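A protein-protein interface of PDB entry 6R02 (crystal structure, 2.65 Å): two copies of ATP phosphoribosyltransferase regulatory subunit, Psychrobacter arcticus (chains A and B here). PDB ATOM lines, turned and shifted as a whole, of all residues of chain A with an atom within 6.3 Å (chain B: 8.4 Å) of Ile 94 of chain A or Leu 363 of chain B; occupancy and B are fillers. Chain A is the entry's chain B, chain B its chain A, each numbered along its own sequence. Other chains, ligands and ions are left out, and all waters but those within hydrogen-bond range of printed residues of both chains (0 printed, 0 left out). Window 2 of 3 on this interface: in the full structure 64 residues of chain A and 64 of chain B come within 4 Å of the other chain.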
ATOM      1  N   GLY A  90     -13.557   5.975  23.421  1.00  0.00           N
ATOM      2  CA  GLY A  90     -14.937   6.079  22.901  1.00  0.00           C
ATOM      3  C   GLY A  90     -15.595   4.736  22.627  1.00  0.00           C
ATOM      4  O   GLY A  90     -16.815   4.644  22.824  1.00  0.00           O
ATOM      5  N   ASP A  92     -16.987   1.611  20.065  1.00  0.00           N
ATOM      6  CA  ASP A  92     -17.726   1.518  18.774  1.00  0.00           C
ATOM      7  C   ASP A  92     -19.104   2.181  18.902  1.00  0.00           C
ATOM      8  O   ASP A  92     -19.660   2.578  17.859  1.00  0.00           O
ATOM      9  CB  ASP A  92     -17.870   0.062  18.317  1.00  0.00           C
ATOM     10  CG  ASP A  92     -16.550  -0.654  18.072  1.00  0.00           C
ATOM     11  OD1 ASP A  92     -15.487  -0.016  18.269  1.00  0.00           O
ATOM     12  OD2 ASP A  92     -16.592  -1.845  17.706  1.00  0.00           O
ATOM     13  N   GLY A  93     -19.641   2.293  20.123  1.00  0.00           N
ATOM     14  CA  GLY A  93     -20.965   2.885  20.390  1.00  0.00           C
ATOM     15  C   GLY A  93     -20.944   4.397  20.235  1.00  0.00           C
ATOM     16  O   GLY A  93     -19.902   4.945  19.833  1.00  0.00           O
ATOM     17  N   ILE A  94     -22.067   5.049  20.530  1.00  0.00           N
ATOM     18  CA  ILE A  94     -22.191   6.534  20.528  1.00  0.00           C
ATOM     19  C   ILE A  94     -21.413   7.072  21.731  1.00  0.00           C
ATOM     20  O   ILE A  94     -21.480   6.444  22.807  1.00  0.00           O
ATOM     21  CB  ILE A  94     -23.671   6.967  20.532  1.00  0.00           C
ATOM     22  CG1 ILE A  94     -24.328   6.652  19.188  1.00  0.00           C
ATOM     23  CG2 ILE A  94     -23.814   8.436  20.898  1.00  0.00           C
ATOM     24  CD1 ILE A  94     -25.831   6.754  19.195  1.00  0.00           C
ATOM     25  N   ALA A  95     -20.680   8.173  21.533  1.00  0.00           N
ATOM     26  CA  ALA A  95     -19.919   8.893  22.575  1.00  0.00           C
ATOM     27  C   ALA A  95     -20.075  10.403  22.365  1.00  0.00           C
ATOM     28  O   ALA A  95     -20.002  10.858  21.203  1.00  0.00           O
ATOM     29  CB  ALA A  95     -18.474   8.482  22.522  1.00  0.00           C
ATOM     30  N   ARG A  96     -20.306  11.138  23.452  1.00  0.00           N
ATOM     31  CA  ARG A  96     -20.471  12.612  23.454  1.00  0.00           C
ATOM     32  C   ARG A  96     -19.322  13.230  24.251  1.00  0.00           C
ATOM     33  O   ARG A  96     -18.929  12.643  25.280  1.00  0.00           O
ATOM     34  CB  ARG A  96     -21.813  13.007  24.079  1.00  0.00           C
ATOM     35  CG  ARG A  96     -23.024  12.377  23.407  1.00  0.00           C
ATOM     36  CD  ARG A  96     -24.304  12.818  24.073  1.00  0.00           C
ATOM     37  NE  ARG A  96     -25.483  12.417  23.328  1.00  0.00           N
ATOM     38  CZ  ARG A  96     -25.992  11.195  23.280  1.00  0.00           C
ATOM     39  NH1 ARG A  96     -25.421  10.208  23.949  1.00  0.00           N
ATOM     40  NH2 ARG A  96     -27.079  10.970  22.560  1.00  0.00           N
ATOM     41  N   ILE A 124     -20.508  14.724  18.858  1.00  0.00           N
ATOM     42  CA  ILE A 124     -21.134  13.370  18.936  1.00  0.00           C
ATOM     43  C   ILE A 124     -20.389  12.470  17.953  1.00  0.00           C
ATOM     44  O   ILE A 124     -20.335  12.825  16.763  1.00  0.00           O
ATOM     45  CB  ILE A 124     -22.646  13.397  18.635  1.00  0.00           C
ATOM     46  CG1 ILE A 124     -23.351  14.522  19.394  1.00  0.00           C
ATOM     47  CG2 ILE A 124     -23.260  12.038  18.923  1.00  0.00           C
ATOM     48  CD1 ILE A 124     -24.851  14.543  19.260  1.00  0.00           C
ATOM     49  N   PHE A 125     -19.828  11.369  18.459  1.00  0.00           N
ATOM     50  CA  PHE A 125     -19.173  10.294  17.674  1.00  0.00           C
ATOM     51  C   PHE A 125     -20.089   9.066  17.675  1.00  0.00           C
ATOM     52  O   PHE A 125     -20.703   8.797  18.722  1.00  0.00           O
ATOM     53  CB  PHE A 125     -17.803   9.956  18.266  1.00  0.00           C
ATOM     54  CG  PHE A 125     -16.720  10.973  18.000  1.00  0.00           C
ATOM     55  CD1 PHE A 125     -16.663  12.159  18.714  1.00  0.00           C
ATOM     56  CD2 PHE A 125     -15.753  10.745  17.038  1.00  0.00           C
ATOM     57  CE1 PHE A 125     -15.669  13.095  18.467  1.00  0.00           C
ATOM     58  CE2 PHE A 125     -14.762  11.682  16.788  1.00  0.00           C
ATOM     59  CZ  PHE A 125     -14.722  12.863  17.494  1.00  0.00           C
ATOM     60  N   GLY A 126     -20.194   8.374  16.535  1.00  0.00           N
ATOM     61  CA  GLY A 126     -20.714   6.995  16.444  1.00  0.00           C
ATOM     62  C   GLY A 126     -22.181   6.909  16.053  1.00  0.00           C
ATOM     63  O   GLY A 126     -22.750   5.811  16.225  1.00  0.00           O
ATOM     64  N   CYS A 127     -22.779   7.986  15.531  1.00  0.00           N
ATOM     65  CA  CYS A 127     -24.191   8.016  15.056  1.00  0.00           C
ATOM     66  C   CYS A 127     -24.264   8.604  13.641  1.00  0.00           C
ATOM     67  O   CYS A 127     -23.785   9.731  13.456  1.00  0.00           O
ATOM     68  CB  CYS A 127     -25.068   8.817  16.010  1.00  0.00           C
ATOM     69  SG  CYS A 127     -26.775   9.020  15.434  1.00  0.00           S
ATOM     70  N   SER A 129     -27.277   8.925  11.889  1.00  0.00           N
ATOM     71  CA  SER A 129     -28.592   9.616  11.819  1.00  0.00           C
ATOM     72  C   SER A 129     -28.408  11.135  11.875  1.00  0.00           C
ATOM     73  O   SER A 129     -27.555  11.600  12.648  1.00  0.00           O
ATOM     74  CB  SER A 129     -29.500   9.152  12.926  1.00  0.00           C
ATOM     75  OG  SER A 129     -30.800   9.708  12.777  1.00  0.00           O
ATOM     76  N   ILE A 130     -29.202  11.869  11.093  1.00  0.00           N
ATOM     77  CA  ILE A 130     -29.361  13.355  11.178  1.00  0.00           C
ATOM     78  C   ILE A 130     -29.852  13.728  12.591  1.00  0.00           C
ATOM     79  O   ILE A 130     -29.761  14.919  12.952  1.00  0.00           O
ATOM     80  CB  ILE A 130     -30.314  13.858  10.071  1.00  0.00           C
ATOM     81  CG1 ILE A 130     -30.265  15.378   9.885  1.00  0.00           C
ATOM     82  CG2 ILE A 130     -31.737  13.378  10.323  1.00  0.00           C
ATOM     83  CD1 ILE A 130     -28.934  15.914   9.412  1.00  0.00           C
ATOM     84  N   ALA A 131     -30.360  12.756  13.356  1.00  0.00           N
ATOM     85  CA  ALA A 131     -30.823  12.917  14.756  1.00  0.00           C
ATOM     86  C   ALA A 131     -29.709  13.495  15.642  1.00  0.00           C
ATOM     87  O   ALA A 131     -30.026  14.324  16.513  1.00  0.00           O
ATOM     88  CB  ALA A 131     -31.308  11.594  15.292  1.00  0.00           C
ATOM     89  N   ALA A 132     -28.461  13.054  15.447  1.00  0.00           N
ATOM     90  CA  ALA A 132     -27.272  13.540  16.190  1.00  0.00           C
ATOM     91  C   ALA A 132     -27.029  15.015  15.858  1.00  0.00           C
ATOM     92  O   ALA A 132     -26.740  15.791  16.769  1.00  0.00           O
ATOM     93  CB  ALA A 132     -26.059  12.701  15.869  1.00  0.00           C
ATOM     94  N   ASP A 133     -27.148  15.385  14.589  1.00  0.00           N
ATOM     95  CA  ASP A 133     -27.018  16.788  14.115  1.00  0.00           C
ATOM     96  C   ASP A 133     -28.141  17.635  14.733  1.00  0.00           C
ATOM     97  O   ASP A 133     -27.901  18.823  14.982  1.00  0.00           O
ATOM     98  CB  ASP A 133     -27.010  16.843  12.589  1.00  0.00           C
ATOM     99  CG  ASP A 133     -25.834  16.110  11.955  1.00  0.00           C
ATOM    100  OD1 ASP A 133     -24.703  16.633  12.036  1.00  0.00           O
ATOM    101  OD2 ASP A 133     -26.053  15.031  11.370  1.00  0.00           O
ATOM    102  N   GLU A 135     -29.702  16.942  17.756  1.00  0.00           N
ATOM    103  CA  GLU A 135     -29.394  17.011  19.208  1.00  0.00           C
ATOM    104  C   GLU A 135     -28.410  18.163  19.479  1.00  0.00           C
ATOM    105  O   GLU A 135     -28.622  18.921  20.448  1.00  0.00           O
ATOM    106  CB  GLU A 135     -28.816  15.686  19.690  1.00  0.00           C
ATOM    107  CG  GLU A 135     -28.453  15.711  21.155  1.00  0.00           C
ATOM    108  CD  GLU A 135     -27.962  14.386  21.701  1.00  0.00           C
ATOM    109  OE1 GLU A 135     -28.574  13.346  21.365  1.00  0.00           O
ATOM    110  OE2 GLU A 135     -26.991  14.408  22.482  1.00  0.00           O
ATOM    111  N   ARG A 303     -15.310   6.103  11.570  1.00  0.00           N
ATOM    112  CA  ARG A 303     -16.156   6.564  12.709  1.00  0.00           C
ATOM    113  C   ARG A 303     -16.927   7.836  12.333  1.00  0.00           C
ATOM    114  O   ARG A 303     -16.299   8.825  11.923  1.00  0.00           O
ATOM    115  CB  ARG A 303     -15.314   6.812  13.963  1.00  0.00           C
ATOM    116  CG  ARG A 303     -16.132   6.998  15.234  1.00  0.00           C
ATOM    117  CD  ARG A 303     -15.604   6.155  16.382  1.00  0.00           C
ATOM    118  NE  ARG A 303     -16.063   6.633  17.679  1.00  0.00           N
ATOM    119  CZ  ARG A 303     -17.173   6.247  18.309  1.00  0.00           C
ATOM    120  NH1 ARG A 303     -17.980   5.344  17.781  1.00  0.00           N
ATOM    121  NH2 ARG A 303     -17.468   6.771  19.487  1.00  0.00           N
ATOM    122  N   LEU B 328     -30.521   8.207  31.744  1.00  0.00           N
ATOM    123  CA  LEU B 328     -30.865   7.847  30.346  1.00  0.00           C
ATOM    124  C   LEU B 328     -32.386   7.726  30.224  1.00  0.00           C
ATOM    125  O   LEU B 328     -32.972   6.878  30.920  1.00  0.00           O
ATOM    126  CB  LEU B 328     -30.181   6.528  29.969  1.00  0.00           C
ATOM    127  CG  LEU B 328     -30.636   5.919  28.643  1.00  0.00           C
ATOM    128  CD1 LEU B 328     -30.441   6.897  27.494  1.00  0.00           C
ATOM    129  CD2 LEU B 328     -29.911   4.615  28.361  1.00  0.00           C
ATOM    130  N   ILE B 329     -32.992   8.540  29.358  1.00  0.00           N
ATOM    131  CA  ILE B 329     -34.425   8.417  28.962  1.00  0.00           C
ATOM    132  C   ILE B 329     -34.580   7.134  28.137  1.00  0.00           C
ATOM    133  O   ILE B 329     -33.767   6.928  27.231  1.00  0.00           O
ATOM    134  CB  ILE B 329     -34.881   9.678  28.200  1.00  0.00           C
ATOM    135  CG1 ILE B 329     -34.952  10.889  29.129  1.00  0.00           C
ATOM    136  CG2 ILE B 329     -36.199   9.452  27.474  1.00  0.00           C
ATOM    137  CD1 ILE B 329     -34.733  12.202  28.437  1.00  0.00           C
ATOM    138  N   TYR B 331     -35.539   4.837  25.298  1.00  0.00           N
ATOM    139  CA  TYR B 331     -35.638   5.139  23.845  1.00  0.00           C
ATOM    140  C   TYR B 331     -37.051   4.828  23.338  1.00  0.00           C
ATOM    141  O   TYR B 331     -37.695   5.728  22.748  1.00  0.00           O
ATOM    142  CB  TYR B 331     -34.580   4.359  23.056  1.00  0.00           C
ATOM    143  CG  TYR B 331     -34.629   4.569  21.563  1.00  0.00           C
ATOM    144  CD1 TYR B 331     -34.282   5.790  20.998  1.00  0.00           C
ATOM    145  CD2 TYR B 331     -35.033   3.554  20.710  1.00  0.00           C
ATOM    146  CE1 TYR B 331     -34.337   5.995  19.628  1.00  0.00           C
ATOM    147  CE2 TYR B 331     -35.087   3.742  19.337  1.00  0.00           C
ATOM    148  CZ  TYR B 331     -34.739   4.967  18.794  1.00  0.00           C
ATOM    149  OH  TYR B 331     -34.787   5.167  17.444  1.00  0.00           O
ATOM    150  N   PHE B 334     -40.101   7.008  24.760  1.00  0.00           N
ATOM    151  CA  PHE B 334     -40.051   8.407  24.258  1.00  0.00           C
ATOM    152  C   PHE B 334     -40.627   8.478  22.837  1.00  0.00           C
ATOM    153  O   PHE B 334     -41.388   9.419  22.548  1.00  0.00           O
ATOM    154  CB  PHE B 334     -38.626   8.968  24.283  1.00  0.00           C
ATOM    155  CG  PHE B 334     -38.517  10.356  23.696  1.00  0.00           C
ATOM    156  CD1 PHE B 334     -39.149  11.434  24.297  1.00  0.00           C
ATOM    157  CD2 PHE B 334     -37.809  10.582  22.527  1.00  0.00           C
ATOM    158  CE1 PHE B 334     -39.078  12.706  23.747  1.00  0.00           C
ATOM    159  CE2 PHE B 334     -37.716  11.858  21.989  1.00  0.00           C
ATOM    160  CZ  PHE B 334     -38.355  12.917  22.595  1.00  0.00           C
ATOM    161  N   ASN B 335     -40.273   7.514  21.982  1.00  0.00           N
ATOM    162  CA  ASN B 335     -40.669   7.487  20.546  1.00  0.00           C
ATOM    163  C   ASN B 335     -42.151   7.114  20.410  1.00  0.00           C
ATOM    164  O   ASN B 335     -42.707   7.345  19.321  1.00  0.00           O
ATOM    165  CB  ASN B 335     -39.774   6.549  19.735  1.00  0.00           C
ATOM    166  CG  ASN B 335     -38.373   7.089  19.565  1.00  0.00           C
ATOM    167  OD1 ASN B 335     -38.177   8.137  18.954  1.00  0.00           O
ATOM    168  ND2 ASN B 335     -37.399   6.383  20.110  1.00  0.00           N
ATOM    169  N   THR B 360     -29.347  12.182  29.192  1.00  0.00           N
ATOM    170  CA  THR B 360     -29.099  11.830  27.771  1.00  0.00           C
ATOM    171  C   THR B 360     -30.432  11.480  27.102  1.00  0.00           C
ATOM    172  O   THR B 360     -31.063  10.490  27.518  1.00  0.00           O
ATOM    173  CB  THR B 360     -28.093  10.677  27.666  1.00  0.00           C
ATOM    174  OG1 THR B 360     -26.878  11.121  28.268  1.00  0.00           O
ATOM    175  CG2 THR B 360     -27.827  10.235  26.247  1.00  0.00           C
ATOM    176  N   MET B 361     -30.838  12.288  26.122  1.00  0.00           N
ATOM    177  CA  MET B 361     -31.936  11.995  25.167  1.00  0.00           C
ATOM    178  C   MET B 361     -31.390  11.064  24.086  1.00  0.00           C
ATOM    179  O   MET B 361     -30.628  11.497  23.223  1.00  0.00           O
ATOM    180  CB  MET B 361     -32.440  13.298  24.536  1.00  0.00           C
ATOM    181  CG  MET B 361     -33.630  13.121  23.607  1.00  0.00           C
ATOM    182  SD  MET B 361     -35.149  12.610  24.461  1.00  0.00           S
ATOM    183  CE  MET B 361     -35.339  13.955  25.634  1.00  0.00           C
ATOM    184  N   PRO B 362     -31.749   9.760  24.092  1.00  0.00           N
ATOM    185  CA  PRO B 362     -31.057   8.766  23.271  1.00  0.00           C
ATOM    186  C   PRO B 362     -31.380   8.829  21.771  1.00  0.00           C
ATOM    187  O   PRO B 362     -32.502   9.134  21.431  1.00  0.00           O
ATOM    188  CB  PRO B 362     -31.556   7.435  23.840  1.00  0.00           C
ATOM    189  CG  PRO B 362     -32.961   7.766  24.290  1.00  0.00           C
ATOM    190  CD  PRO B 362     -32.862   9.173  24.852  1.00  0.00           C
ATOM    191  N   LEU B 363     -30.379   8.540  20.931  1.00  0.00           N
ATOM    192  CA  LEU B 363     -30.466   8.531  19.445  1.00  0.00           C
ATOM    193  C   LEU B 363     -30.836   7.124  18.951  1.00  0.00           C
ATOM    194  O   LEU B 363     -31.394   7.018  17.846  1.00  0.00           O
ATOM    195  CB  LEU B 363     -29.121   8.981  18.866  1.00  0.00           C
ATOM    196  CG  LEU B 363     -28.704  10.413  19.203  1.00  0.00           C
ATOM    197  CD1 LEU B 363     -27.201  10.590  19.086  1.00  0.00           C
ATOM    198  CD2 LEU B 363     -29.424  11.422  18.325  1.00  0.00           C
ATOM    199  N   THR B 364     -30.506   6.086  19.729  1.00  0.00           N
ATOM    200  CA  THR B 364     -30.763   4.651  19.420  1.00  0.00           C
ATOM    201  C   THR B 364     -31.064   3.891  20.716  1.00  0.00           C
ATOM    202  O   THR B 364     -30.797   4.438  21.800  1.00  0.00           O
ATOM    203  CB  THR B 364     -29.576   4.014  18.683  1.00  0.00           C
ATOM    204  OG1 THR B 364     -28.543   3.720  19.623  1.00  0.00           O
ATOM    205  CG2 THR B 364     -29.015   4.886  17.581  1.00  0.00           C
ATOM    206  N   ALA B 365     -31.579   2.666  20.600  1.00  0.00           N
ATOM    207  CA  ALA B 365     -31.893   1.752  21.724  1.00  0.00           C
ATOM    208  C   ALA B 365     -30.620   1.390  22.501  1.00  0.00           C
ATOM    209  O   ALA B 365     -30.748   0.993  23.673  1.00  0.00           O
ATOM    210  CB  ALA B 365     -32.569   0.508  21.199  1.00  0.00           C
ATOM    211  N   GLU B 366     -29.445   1.501  21.868  1.00  0.00           N
ATOM    212  CA  GLU B 366     -28.138   1.063  22.433  1.00  0.00           C
ATOM    213  C   GLU B 366     -27.380   2.259  23.023  1.00  0.00           C
ATOM    214  O   GLU B 366     -26.426   2.014  23.783  1.00  0.00           O
ATOM    215  CB  GLU B 366     -27.287   0.374  21.362  1.00  0.00           C
ATOM    216  CG  GLU B 366     -27.998  -0.776  20.659  1.00  0.00           C
ATOM    217  CD  GLU B 366     -28.812  -0.379  19.435  1.00  0.00           C
ATOM    218  OE1 GLU B 366     -28.343   0.491  18.670  1.00  0.00           O
ATOM    219  OE2 GLU B 366     -29.909  -0.941  19.247  1.00  0.00           O
ATOM    220  N   ASP B 367     -27.790   3.491  22.690  1.00  0.00           N
ATOM    221  CA  ASP B 367     -27.192   4.761  23.185  1.00  0.00           C
ATOM    222  C   ASP B 367     -27.125   4.711  24.716  1.00  0.00           C
ATOM    223  O   ASP B 367     -28.167   4.900  25.359  1.00  0.00           O
ATOM    224  CB  ASP B 367     -27.991   5.968  22.683  1.00  0.00           C
ATOM    225  CG  ASP B 367     -27.322   7.316  22.895  1.00  0.00           C
ATOM    226  OD1 ASP B 367     -26.361   7.388  23.684  1.00  0.00           O
ATOM    227  OD2 ASP B 367     -27.776   8.295  22.266  1.00  0.00           O
ATOM    228  N   MET B 368     -25.934   4.460  25.264  1.00  0.00           N
ATOM    229  CA  MET B 368     -25.692   4.239  26.716  1.00  0.00           C
ATOM    230  C   MET B 368     -24.696   5.283  27.220  1.00  0.00           C
ATOM    231  O   MET B 368     -23.529   5.254  26.837  1.00  0.00           O
ATOM    232  CB  MET B 368     -25.122   2.841  26.971  1.00  0.00           C
ATOM    233  CG  MET B 368     -25.283   2.399  28.403  1.00  0.00           C
ATOM    234  SD  MET B 368     -26.858   1.525  28.572  1.00  0.00           S
ATOM    235  CE  MET B 368     -26.560   0.105  27.516  1.00  0.00           C
ATOM    236  N   PRO B 369     -25.111   6.237  28.087  1.00  0.00           N
ATOM    237  CA  PRO B 369     -24.165   7.124  28.761  1.00  0.00           C
ATOM    238  C   PRO B 369     -23.178   6.352  29.651  1.00  0.00           C
ATOM    239  O   PRO B 369     -23.560   5.337  30.233  1.00  0.00           O
ATOM    240  CB  PRO B 369     -25.050   8.032  29.628  1.00  0.00           C
ATOM    241  CG  PRO B 369     -26.424   7.928  29.009  1.00  0.00           C
ATOM    242  CD  PRO B 369     -26.506   6.526  28.446  1.00  0.00           C
ATOM    243  N   VAL B 370     -21.943   6.850  29.743  1.00  0.00           N
ATOM    244  CA  VAL B 370     -20.867   6.248  30.582  1.00  0.00           C
ATOM    245  C   VAL B 370     -21.262   6.439  32.053  1.00  0.00           C
ATOM    246  O   VAL B 370     -21.737   7.538  32.393  1.00  0.00           O
ATOM    247  CB  VAL B 370     -19.490   6.871  30.268  1.00  0.00           C
ATOM    248  CG1 VAL B 370     -18.389   6.292  31.142  1.00  0.00           C
ATOM    249  CG2 VAL B 370     -19.127   6.734  28.797  1.00  0.00           C
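No residue of chain B comes within 4 Å of Gly 93 of chain A.
Of the printed residues of chain B, Ile 94 of chain A touches Leu 363 and Asp 367.
Printed residues of chain B within 4 Å of Arg 96 of chain A: Thr 360 (3.3 Å), Met 361 (3.6 Å), Leu 363 (3.5 Å) and Asp 367 (2.8 Å).
Of the printed residues of chain B, Cys 127 of chain A touches Leu 363 (3.998 Å).
Printed residues of chain B within 4 Å of Ala 132 of chain A: Leu 363 (3.4 Å).
Tyr 331 of chain B touches none of the printed residues of chain A.
Of the printed residues of chain A, Met 361 of chain B touches Arg 96 (3.6 Å) and Glu 135 (3.3 Å).
The nearest printed residue of chain A that does not touch Leu 363 of chain B is Ile 124 of chain A (4.2 Å).
The nearest printed residue of chain A that does not touch Thr 360 of chain B is Glu 135 of chain A (5.7 Å).
Of the 17 printed residues of chain A, 6 touch a printed residue of chain B.
Hydrophobic or aromatic side chains of chain A within 4 Å of the printed part of chain B: Ile 94 and Ala 131.
Of the 16 printed residues of chain B, 4 touch a printed residue of chain A.
Hydrophobic or aromatic side chains of chain B that line the printed part of chain A: Leu 363.
Among the printed residues, 11 pairs touch across the chains.
Among the printed residues, Asp or Glu carboxylates within 4 Å of a Lys or Arg side-chain nitrogen of the other chain: Arg 96 of chain A with Asp 367 of chain B.
No position is printed for both chains.
N of Ile 329 of chain B lies within hydrogen-bond range of O of Thr 360 of chain B (3.3 Å).
N of Leu 363 of chain B is in hydrogen-bond range of OD2 of Asp 367 of chain B (2.9 Å).
The backbone NH of Asp 367 of chain B lies within hydrogen-bond range of the side-chain hydroxyl of Thr 364 of chain B (3.2 Å).
The side-chain carboxylate (OE2) of Glu 135 of chain A lies within salt-bridge range of the guanidinium group (NE) of Arg 96 of chain A, at 2.6 Å.
SG of Cys 127 of chain A sits close to N of Ser 129 of chain A (3.6 Å).
N of Ala 131 of chain A sits close to OG of Ser 129 of chain A (3.1 Å).
Among the printed residues, pairs that only touch across the chains: Arg 96 of chain A with Thr 360 of chain B (3.3 Å), Ala 131 of chain A with Leu 363 of chain B (3.4 Å), Ala 132 of chain A with Leu 363 of chain B (3.4 Å), Arg 96 of chain A with Leu 363 of chain B (3.5 Å), Glu 135 of chain A with Leu 363 of chain B (3.6 Å), Arg 96 of chain A with Met 361 of chain B (3.6 Å), Ile 94 of chain A with Asp 367 of chain B (3.9 Å), Ile 94 of chain A with Leu 363 of chain B (3.99 Å) and Cys 127 of chain A with Leu 363 of chain B (3.998 Å).
OD2 of Asp 367 of chain B lies within salt-bridge range of NH2 of Arg 96 of chain A, 2.8 Å away.
The side-chain carboxylate (OE1) of Glu 135 of chain A lies close to the backbone carbonyl oxygen (O) of Met 361 of chain B.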
